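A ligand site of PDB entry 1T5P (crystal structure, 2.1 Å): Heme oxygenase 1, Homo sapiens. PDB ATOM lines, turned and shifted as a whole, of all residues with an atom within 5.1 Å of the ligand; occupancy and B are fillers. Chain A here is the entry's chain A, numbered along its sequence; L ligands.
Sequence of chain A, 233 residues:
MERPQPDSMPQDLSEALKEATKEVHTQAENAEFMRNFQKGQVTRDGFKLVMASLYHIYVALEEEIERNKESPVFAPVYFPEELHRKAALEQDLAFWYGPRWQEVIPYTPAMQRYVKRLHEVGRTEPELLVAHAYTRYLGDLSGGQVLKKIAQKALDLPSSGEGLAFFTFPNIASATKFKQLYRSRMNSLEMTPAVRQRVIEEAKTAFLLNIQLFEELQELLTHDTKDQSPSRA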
ATOM      1  N   SER A  14     -11.107   5.767  19.469  1.00  0.00           N
ATOM      2  CA  SER A  14     -12.070   6.831  19.725  1.00  0.00           C
ATOM      3  C   SER A  14     -13.361   6.595  18.961  1.00  0.00           C
ATOM      4  O   SER A  14     -14.458   6.645  19.522  1.00  0.00           O
ATOM      5  CB  SER A  14     -11.460   8.170  19.312  1.00  0.00           C
ATOM      6  OG  SER A  14     -12.467   9.150  19.199  1.00  0.00           O
ATOM      7  N   LYS A  18     -17.201   5.495  20.372  1.00  0.00           N
ATOM      8  CA  LYS A  18     -18.394   6.267  20.056  1.00  0.00           C
ATOM      9  C   LYS A  18     -19.501   5.366  19.502  1.00  0.00           C
ATOM     10  O   LYS A  18     -20.652   5.425  19.969  1.00  0.00           O
ATOM     11  CB  LYS A  18     -18.084   7.363  19.027  1.00  0.00           C
ATOM     12  CG  LYS A  18     -19.345   8.003  18.442  1.00  0.00           C
ATOM     13  CD  LYS A  18     -19.669   9.341  19.078  1.00  0.00           C
ATOM     14  CE  LYS A  18     -18.616  10.370  18.731  1.00  0.00           C
ATOM     15  NZ  LYS A  18     -18.337  10.375  17.266  1.00  0.00           N
ATOM     16  N   THR A  21     -20.966   3.006  22.067  1.00  0.00           N
ATOM     17  CA  THR A  21     -21.796   3.736  23.021  1.00  0.00           C
ATOM     18  C   THR A  21     -22.942   4.487  22.360  1.00  0.00           C
ATOM     19  O   THR A  21     -23.369   5.545  22.831  1.00  0.00           O
ATOM     20  CB  THR A  21     -20.960   4.756  23.831  1.00  0.00           C
ATOM     21  OG1 THR A  21     -20.499   5.802  22.975  1.00  0.00           O
ATOM     22  CG2 THR A  21     -19.779   4.065  24.480  1.00  0.00           C
ATOM     23  N   HIS A  25     -26.601   4.062  24.078  1.00  0.00           N
ATOM     24  CA  HIS A  25     -26.829   5.418  24.554  1.00  0.00           C
ATOM     25  C   HIS A  25     -28.275   5.857  24.352  1.00  0.00           C
ATOM     26  O   HIS A  25     -28.570   7.051  24.275  1.00  0.00           O
ATOM     27  CB  HIS A  25     -25.887   6.382  23.815  1.00  0.00           C
ATOM     28  CG  HIS A  25     -25.698   7.703  24.502  1.00  0.00           C
ATOM     29  ND1 HIS A  25     -26.704   8.627  24.639  1.00  0.00           N
ATOM     30  CD2 HIS A  25     -24.600   8.239  25.079  1.00  0.00           C
ATOM     31  CE1 HIS A  25     -26.242   9.683  25.275  1.00  0.00           C
ATOM     32  NE2 HIS A  25     -24.970   9.483  25.550  1.00  0.00           N
ATOM     33  N   THR A  26     -29.189   4.896  24.277  1.00  0.00           N
ATOM     34  CA  THR A  26     -30.596   5.220  24.089  1.00  0.00           C
ATOM     35  C   THR A  26     -31.413   4.615  25.209  1.00  0.00           C
ATOM     36  O   THR A  26     -32.472   5.135  25.585  1.00  0.00           O
ATOM     37  CB  THR A  26     -31.100   4.680  22.732  1.00  0.00           C
ATOM     38  OG1 THR A  26     -30.239   5.148  21.674  1.00  0.00           O
ATOM     39  CG2 THR A  26     -32.507   5.154  22.454  1.00  0.00           C
ATOM     40  N   GLN A  27     -30.911   3.509  25.759  1.00  0.00           N
ATOM     41  CA  GLN A  27     -31.585   2.800  26.827  1.00  0.00           C
ATOM     42  C   GLN A  27     -31.764   3.606  28.108  1.00  0.00           C
ATOM     43  O   GLN A  27     -31.015   4.554  28.379  1.00  0.00           O
ATOM     44  CB  GLN A  27     -30.822   1.525  27.170  1.00  0.00           C
ATOM     45  CG  GLN A  27     -30.697   0.508  26.055  1.00  0.00           C
ATOM     46  CD  GLN A  27     -29.898  -0.706  26.491  1.00  0.00           C
ATOM     47  OE1 GLN A  27     -30.175  -1.304  27.536  1.00  0.00           O
ATOM     48  NE2 GLN A  27     -28.901  -1.083  25.705  1.00  0.00           N
ATOM     49  N   ALA A  28     -32.758   3.198  28.883  1.00  0.00           N
ATOM     50  CA  ALA A  28     -33.084   3.801  30.167  1.00  0.00           C
ATOM     51  C   ALA A  28     -33.710   5.197  30.144  1.00  0.00           C
ATOM     52  O   ALA A  28     -33.190   6.127  30.764  1.00  0.00           O
ATOM     53  CB  ALA A  28     -31.838   3.795  31.065  1.00  0.00           C
ATOM     54  N   GLU A  29     -34.808   5.356  29.407  1.00  0.00           N
ATOM     55  CA  GLU A  29     -35.467   6.648  29.378  1.00  0.00           C
ATOM     56  C   GLU A  29     -36.596   6.519  30.399  1.00  0.00           C
ATOM     57  O   GLU A  29     -37.668   7.127  30.263  1.00  0.00           O
ATOM     58  CB  GLU A  29     -36.067   6.945  27.990  1.00  0.00           C
ATOM     59  CG  GLU A  29     -35.263   6.417  26.814  1.00  0.00           C
ATOM     60  CD  GLU A  29     -35.639   4.987  26.460  1.00  0.00           C
ATOM     61  OE1 GLU A  29     -35.261   4.531  25.357  1.00  0.00           O
ATOM     62  OE2 GLU A  29     -36.296   4.324  27.281  1.00  0.00           O
ATOM     63  N   TYR A 134     -13.254   7.852  29.817  1.00  0.00           N
ATOM     64  CA  TYR A 134     -13.943   8.338  28.638  1.00  0.00           C
ATOM     65  C   TYR A 134     -15.453   8.513  28.875  1.00  0.00           C
ATOM     66  O   TYR A 134     -16.031   9.580  28.627  1.00  0.00           O
ATOM     67  CB  TYR A 134     -13.709   7.348  27.507  1.00  0.00           C
ATOM     68  CG  TYR A 134     -14.613   7.548  26.331  1.00  0.00           C
ATOM     69  CD1 TYR A 134     -14.297   8.475  25.346  1.00  0.00           C
ATOM     70  CD2 TYR A 134     -15.790   6.806  26.195  1.00  0.00           C
ATOM     71  CE1 TYR A 134     -15.143   8.671  24.251  1.00  0.00           C
ATOM     72  CE2 TYR A 134     -16.632   6.989  25.104  1.00  0.00           C
ATOM     73  CZ  TYR A 134     -16.306   7.917  24.139  1.00  0.00           C
ATOM     74  OH  TYR A 134     -17.143   8.093  23.071  1.00  0.00           O
ATOM     75  N   THR A 135     -16.076   7.433  29.343  1.00  0.00           N
ATOM     76  CA  THR A 135     -17.507   7.408  29.627  1.00  0.00           C
ATOM     77  C   THR A 135     -17.900   8.548  30.543  1.00  0.00           C
ATOM     78  O   THR A 135     -18.855   9.284  30.283  1.00  0.00           O
ATOM     79  CB  THR A 135     -17.872   6.106  30.305  1.00  0.00           C
ATOM     80  OG1 THR A 135     -17.347   5.024  29.528  1.00  0.00           O
ATOM     81  CG2 THR A 135     -19.372   5.945  30.406  1.00  0.00           C
ATOM     82  N   ARG A 136     -17.147   8.659  31.630  1.00  0.00           N
ATOM     83  CA  ARG A 136     -17.372   9.683  32.634  1.00  0.00           C
ATOM     84  C   ARG A 136     -17.085  11.105  32.123  1.00  0.00           C
ATOM     85  O   ARG A 136     -17.998  11.911  31.954  1.00  0.00           O
ATOM     86  CB  ARG A 136     -16.497   9.354  33.843  1.00  0.00           C
ATOM     87  CG  ARG A 136     -17.110   9.639  35.198  1.00  0.00           C
ATOM     88  CD  ARG A 136     -18.483   9.028  35.340  1.00  0.00           C
ATOM     89  NE  ARG A 136     -19.530   9.938  34.905  1.00  0.00           N
ATOM     90  CZ  ARG A 136     -20.819   9.641  34.907  1.00  0.00           C
ATOM     91  NH1 ARG A 136     -21.214   8.446  35.332  1.00  0.00           N
ATOM     92  NH2 ARG A 136     -21.717  10.536  34.508  1.00  0.00           N
ATOM     93  N   LEU A 138     -15.804  12.529  28.999  1.00  0.00           N
ATOM     94  CA  LEU A 138     -16.368  12.998  27.743  1.00  0.00           C
ATOM     95  C   LEU A 138     -17.885  12.978  27.768  1.00  0.00           C
ATOM     96  O   LEU A 138     -18.529  13.814  27.148  1.00  0.00           O
ATOM     97  CB  LEU A 138     -15.847  12.183  26.555  1.00  0.00           C
ATOM     98  CG  LEU A 138     -14.359  12.365  26.226  1.00  0.00           C
ATOM     99  CD1 LEU A 138     -14.138  12.114  24.732  1.00  0.00           C
ATOM    100  CD2 LEU A 138     -13.886  13.766  26.593  1.00  0.00           C
ATOM    101  N   GLY A 139     -18.463  12.024  28.487  1.00  0.00           N
ATOM    102  CA  GLY A 139     -19.905  11.987  28.587  1.00  0.00           C
ATOM    103  C   GLY A 139     -20.428  13.227  29.301  1.00  0.00           C
ATOM    104  O   GLY A 139     -21.297  13.924  28.773  1.00  0.00           O
ATOM    105  N   SER A 142     -19.689  16.936  27.220  1.00  0.00           N
ATOM    106  CA  SER A 142     -20.586  17.312  26.135  1.00  0.00           C
ATOM    107  C   SER A 142     -22.073  17.219  26.476  1.00  0.00           C
ATOM    108  O   SER A 142     -22.893  17.856  25.828  1.00  0.00           O
ATOM    109  CB  SER A 142     -20.276  16.480  24.894  1.00  0.00           C
ATOM    110  OG  SER A 142     -20.328  15.089  25.167  1.00  0.00           O
ATOM    111  N   GLY A 143     -22.418  16.428  27.484  1.00  0.00           N
ATOM    112  CA  GLY A 143     -23.812  16.280  27.857  1.00  0.00           C
ATOM    113  C   GLY A 143     -24.265  17.310  28.876  1.00  0.00           C
ATOM    114  O   GLY A 143     -25.446  17.639  28.965  1.00  0.00           O
ATOM    115  N   VAL A 146     -26.721  20.370  28.382  1.00  0.00           N
ATOM    116  CA  VAL A 146     -28.056  19.837  28.232  1.00  0.00           C
ATOM    117  C   VAL A 146     -28.578  19.530  29.645  1.00  0.00           C
ATOM    118  O   VAL A 146     -29.452  20.223  30.161  1.00  0.00           O
ATOM    119  CB  VAL A 146     -28.042  18.526  27.400  1.00  0.00           C
ATOM    120  CG1 VAL A 146     -29.436  17.938  27.304  1.00  0.00           C
ATOM    121  CG2 VAL A 146     -27.481  18.804  26.005  1.00  0.00           C
ATOM    122  N   LEU A 147     -28.006  18.496  30.240  1.00  0.00           N
ATOM    123  CA  LEU A 147     -28.384  18.039  31.574  1.00  0.00           C
ATOM    124  C   LEU A 147     -28.453  19.165  32.607  1.00  0.00           C
ATOM    125  O   LEU A 147     -29.016  18.990  33.685  1.00  0.00           O
ATOM    126  CB  LEU A 147     -27.391  16.975  32.031  1.00  0.00           C
ATOM    127  CG  LEU A 147     -27.054  15.897  30.994  1.00  0.00           C
ATOM    128  CD1 LEU A 147     -25.861  15.069  31.455  1.00  0.00           C
ATOM    129  CD2 LEU A 147     -28.277  15.011  30.760  1.00  0.00           C
ATOM    130  N   LYS A 179     -11.950  17.789  23.374  1.00  0.00           N
ATOM    131  CA  LYS A 179     -12.408  16.467  22.949  1.00  0.00           C
ATOM    132  C   LYS A 179     -11.522  15.911  21.829  1.00  0.00           C
ATOM    133  O   LYS A 179     -11.181  14.723  21.827  1.00  0.00           O
ATOM    134  CB  LYS A 179     -13.852  16.548  22.473  1.00  0.00           C
ATOM    135  CG  LYS A 179     -14.848  16.978  23.536  1.00  0.00           C
ATOM    136  CD  LYS A 179     -16.188  17.323  22.915  1.00  0.00           C
ATOM    137  CE  LYS A 179     -17.328  16.875  23.777  1.00  0.00           C
ATOM    138  NZ  LYS A 179     -17.291  15.381  23.981  1.00  0.00           N
ATOM    139  N   ARG A 183      -9.537  12.647  22.235  1.00  0.00           N
ATOM    140  CA  ARG A 183      -9.730  11.493  21.367  1.00  0.00           C
ATOM    141  C   ARG A 183      -8.409  11.087  20.725  1.00  0.00           C
ATOM    142  O   ARG A 183      -8.105   9.892  20.612  1.00  0.00           O
ATOM    143  CB  ARG A 183     -10.771  11.793  20.274  1.00  0.00           C
ATOM    144  CG  ARG A 183     -12.168  12.118  20.770  1.00  0.00           C
ATOM    145  CD  ARG A 183     -13.171  11.921  19.645  1.00  0.00           C
ATOM    146  NE  ARG A 183     -14.190  12.958  19.504  1.00  0.00           N
ATOM    147  CZ  ARG A 183     -15.103  13.261  20.423  1.00  0.00           C
ATOM    148  NH1 ARG A 183     -15.145  12.611  21.572  1.00  0.00           N
ATOM    149  NH2 ARG A 183     -16.018  14.193  20.160  1.00  0.00           N
ATOM    150  N   ALA A 206     -19.588   0.143  31.772  1.00  0.00           N
ATOM    151  CA  ALA A 206     -19.769   1.416  32.461  1.00  0.00           C
ATOM    152  C   ALA A 206     -21.160   1.988  32.213  1.00  0.00           C
ATOM    153  O   ALA A 206     -21.710   2.707  33.056  1.00  0.00           O
ATOM    154  CB  ALA A 206     -18.720   2.402  32.023  1.00  0.00           C
ATOM    155  N   PHE A 207     -21.727   1.700  31.043  1.00  0.00           N
ATOM    156  CA  PHE A 207     -23.068   2.202  30.719  1.00  0.00           C
ATOM    157  C   PHE A 207     -24.112   1.432  31.487  1.00  0.00           C
ATOM    158  O   PHE A 207     -25.156   1.980  31.863  1.00  0.00           O
ATOM    159  CB  PHE A 207     -23.338   2.121  29.228  1.00  0.00           C
ATOM    160  CG  PHE A 207     -22.770   3.254  28.452  1.00  0.00           C
ATOM    161  CD1 PHE A 207     -21.385   3.364  28.291  1.00  0.00           C
ATOM    162  CD2 PHE A 207     -23.593   4.238  27.913  1.00  0.00           C
ATOM    163  CE1 PHE A 207     -20.832   4.444  27.608  1.00  0.00           C
ATOM    164  CE2 PHE A 207     -23.059   5.324  27.218  1.00  0.00           C
ATOM    165  CZ  PHE A 207     -21.673   5.436  27.067  1.00  0.00           C
ATOM    166  N   ASN A 210     -24.104   2.685  35.022  1.00  0.00           N
ATOM    167  CA  ASN A 210     -24.758   3.980  35.076  1.00  0.00           C
ATOM    168  C   ASN A 210     -26.251   3.769  34.951  1.00  0.00           C
ATOM    169  O   ASN A 210     -27.038   4.385  35.665  1.00  0.00           O
ATOM    170  CB  ASN A 210     -24.263   4.896  33.954  1.00  0.00           C
ATOM    171  CG  ASN A 210     -23.016   5.668  34.349  1.00  0.00           C
ATOM    172  OD1 ASN A 210     -23.074   6.622  35.132  1.00  0.00           O
ATOM    173  ND2 ASN A 210     -21.864   5.248  33.829  1.00  0.00           N
ATOM    174  N   PHE A 214     -29.238   4.629  37.837  1.00  0.00           N
ATOM    175  CA  PHE A 214     -30.471   5.401  37.692  1.00  0.00           C
ATOM    176  C   PHE A 214     -31.677   4.526  38.011  1.00  0.00           C
ATOM    177  O   PHE A 214     -32.647   4.996  38.596  1.00  0.00           O
ATOM    178  CB  PHE A 214     -30.595   5.949  36.261  1.00  0.00           C
ATOM    179  CG  PHE A 214     -29.396   6.748  35.819  1.00  0.00           C
ATOM    180  CD1 PHE A 214     -28.900   7.775  36.631  1.00  0.00           C
ATOM    181  CD2 PHE A 214     -28.740   6.450  34.634  1.00  0.00           C
ATOM    182  CE1 PHE A 214     -27.762   8.497  36.250  1.00  0.00           C
ATOM    183  CE2 PHE A 214     -27.599   7.153  34.237  1.00  0.00           C
ATOM    184  CZ  PHE A 214     -27.102   8.183  35.059  1.00  0.00           C
HETATM  185 FE1  LIG L   1     -24.545  11.198  27.062  1.00  0.00          FE
HETATM  186  N1  LIG L   1     -24.422  12.691  25.751  1.00  0.00           N
HETATM  187  N2  LIG L   1     -26.402  11.833  27.565  1.00  0.00           N
HETATM  188  N3  LIG L   1     -24.607   9.750  28.364  1.00  0.00           N
HETATM  189  N4  LIG L   1     -22.657  10.650  26.517  1.00  0.00           N
HETATM  190  C1  LIG L   1     -23.356  13.046  24.882  1.00  0.00           C
HETATM  191  C2  LIG L   1     -22.135  12.335  24.809  1.00  0.00           C
HETATM  192  C3  LIG L   1     -21.828  11.246  25.557  1.00  0.00           C
HETATM  193  C4  LIG L   1     -27.088  12.936  27.009  1.00  0.00           C
HETATM  194  C5  LIG L   1     -26.603  13.761  26.055  1.00  0.00           C
HETATM  195  C6  LIG L   1     -25.371  13.660  25.468  1.00  0.00           C
HETATM  196  C7  LIG L   1     -25.681   9.385  29.257  1.00  0.00           C
HETATM  197  C8  LIG L   1     -26.980  10.103  29.356  1.00  0.00           C
HETATM  198  C9  LIG L   1     -27.300  11.279  28.527  1.00  0.00           C
HETATM  199  C10 LIG L   1     -21.885   9.606  27.005  1.00  0.00           C
HETATM  200  C11 LIG L   1     -22.326   8.760  27.974  1.00  0.00           C
HETATM  201  C12 LIG L   1     -23.585   8.822  28.607  1.00  0.00           C
HETATM  202  C13 LIG L   1     -23.660  14.269  24.038  1.00  0.00           C
HETATM  203  C14 LIG L   1     -22.802  14.998  22.959  1.00  0.00           C
HETATM  204  C15 LIG L   1     -24.914  14.624  24.418  1.00  0.00           C
HETATM  205  C16 LIG L   1     -25.668  15.845  23.808  1.00  0.00           C
HETATM  206  C17 LIG L   1     -22.464  14.210  21.682  1.00  0.00           C
HETATM  207  C18 LIG L   1     -20.953  14.184  21.355  1.00  0.00           C
HETATM  208  O1  LIG L   1     -20.280  15.259  21.485  1.00  0.00           O
HETATM  209  O2  LIG L   1     -20.442  13.107  20.968  1.00  0.00           O
HETATM  210  C19 LIG L   1     -28.396  13.145  27.567  1.00  0.00           C
HETATM  211  C20 LIG L   1     -29.408  14.273  27.185  1.00  0.00           C
HETATM  212  C21 LIG L   1     -28.583  12.153  28.511  1.00  0.00           C
HETATM  213  C22 LIG L   1     -29.772  12.073  29.269  1.00  0.00           C
HETATM  214  C23 LIG L   1     -30.992  11.436  28.786  1.00  0.00           C
HETATM  215  C24 LIG L   1     -25.246   8.185  30.074  1.00  0.00           C
HETATM  216  C25 LIG L   1     -25.953   7.342  31.188  1.00  0.00           C
HETATM  217  C26 LIG L   1     -23.987   7.892  29.642  1.00  0.00           C
HETATM  218  C27 LIG L   1     -23.197   6.841  30.142  1.00  0.00           C
HETATM  219  C28 LIG L   1     -22.307   7.202  31.233  1.00  0.00           C
HETATM  220  C29 LIG L   1     -20.579   9.541  26.338  1.00  0.00           C
HETATM  221  C30 LIG L   1     -19.431   8.568  26.565  1.00  0.00           C
HETATM  222  C31 LIG L   1     -20.540  10.564  25.438  1.00  0.00           C
HETATM  223  C32 LIG L   1     -19.391  10.951  24.490  1.00  0.00           C
HETATM  224  C33 LIG L   1     -19.265  10.436  23.055  1.00  0.00           C
HETATM  225  C34 LIG L   1     -18.005  11.010  22.365  1.00  0.00           C
HETATM  226  O3  LIG L   1     -17.236  10.211  21.754  1.00  0.00           O
HETATM  227  O4  LIG L   1     -17.791  12.260  22.432  1.00  0.00           O
HETATM  228  C35 LIG L   1     -28.192   9.168  29.305  1.00  0.00           C
HETATM  229  C36 LIG L   1     -28.670   8.538  28.111  1.00  0.00           C
HETATM  230  C37 LIG L   1     -28.891   8.903  30.549  1.00  0.00           C
HETATM  231  C38 LIG L   1     -29.804   7.679  28.157  1.00  0.00           C
HETATM  232  C39 LIG L   1     -29.994   8.052  30.568  1.00  0.00           C
HETATM  233  C40 LIG L   1     -30.467   7.434  29.381  1.00  0.00           C
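A ring nitrogen (NE2) of His 25 is bound to an iron atom (FE1) of the ligand, 2.3 Å away.
OH of Tyr 134 lies within hydrogen-bond range of O3 of the ligand, at 2.5 Å.
The side-chain amino group (NZ) of Lys 179 is in salt-bridge range of an oxygen (O4) of the ligand (3.5 Å).
NH1 of Arg 183 is in salt-bridge range of O4 of the ligand, at 2.8 Å.
The side-chain hydroxyl of Ser 142 lies within hydrogen-bond range of the backbone carbonyl oxygen of Leu 138.
The side-chain hydroxyl (OG1) of Thr 21 is in hydrogen-bond range of the backbone carbonyl oxygen (O) of Lys 18 (3.0 Å).
OD1 of Asn 210 is in hydrogen-bond range of NH1 of Arg 136, 2.6 Å away.
The backbone carbonyl oxygen (O) of Tyr 134 sits at hydrogen-bond distance from the backbone NH (N) of Gly 139 (3.5 Å).
The side-chain amide nitrogen (ND2) of Asn 210 is in hydrogen-bond range of the backbone carbonyl oxygen (O) of Ala 206, 2.7 Å away.
The side-chain hydroxyl (OG) of Ser 142 sits at hydrogen-bond distance from the side-chain amino group (NZ) of Lys 179, at 3.3 Å.
Residues that only touch the ligand: Lys 18 (3.3 Å), Gln 27 (3.1 Å), Ala 28 (3.3 Å), Thr 135 (3.3 Å), Gly 139 (3.4 Å), Ser 142 (3.3 Å), Gly 143 (3.9 Å), Val 146 (3.7 Å), Leu 147 (3.6 Å), Phe 207 (3.3 Å), Asn 210 (3.3 Å) and Phe 214 (3.5 Å).
Hydrophobic or aromatic side chains within 4 Å of the ligand: His 25, Tyr 134, Val 146, Leu 147, Phe 207 and Phe 214.
16 residues have an atom within 4 Å of the ligand: Lys 18, His 25, Gln 27, Ala 28, Tyr 134, Thr 135, Gly 139, Ser 142, Gly 143, Val 146, Leu 147, Lys 179, Arg 183, Phe 207, Asn 210 and Phe 214.
The nearest printed residue that does not touch the ligand is Leu 138 (4.001 Å).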
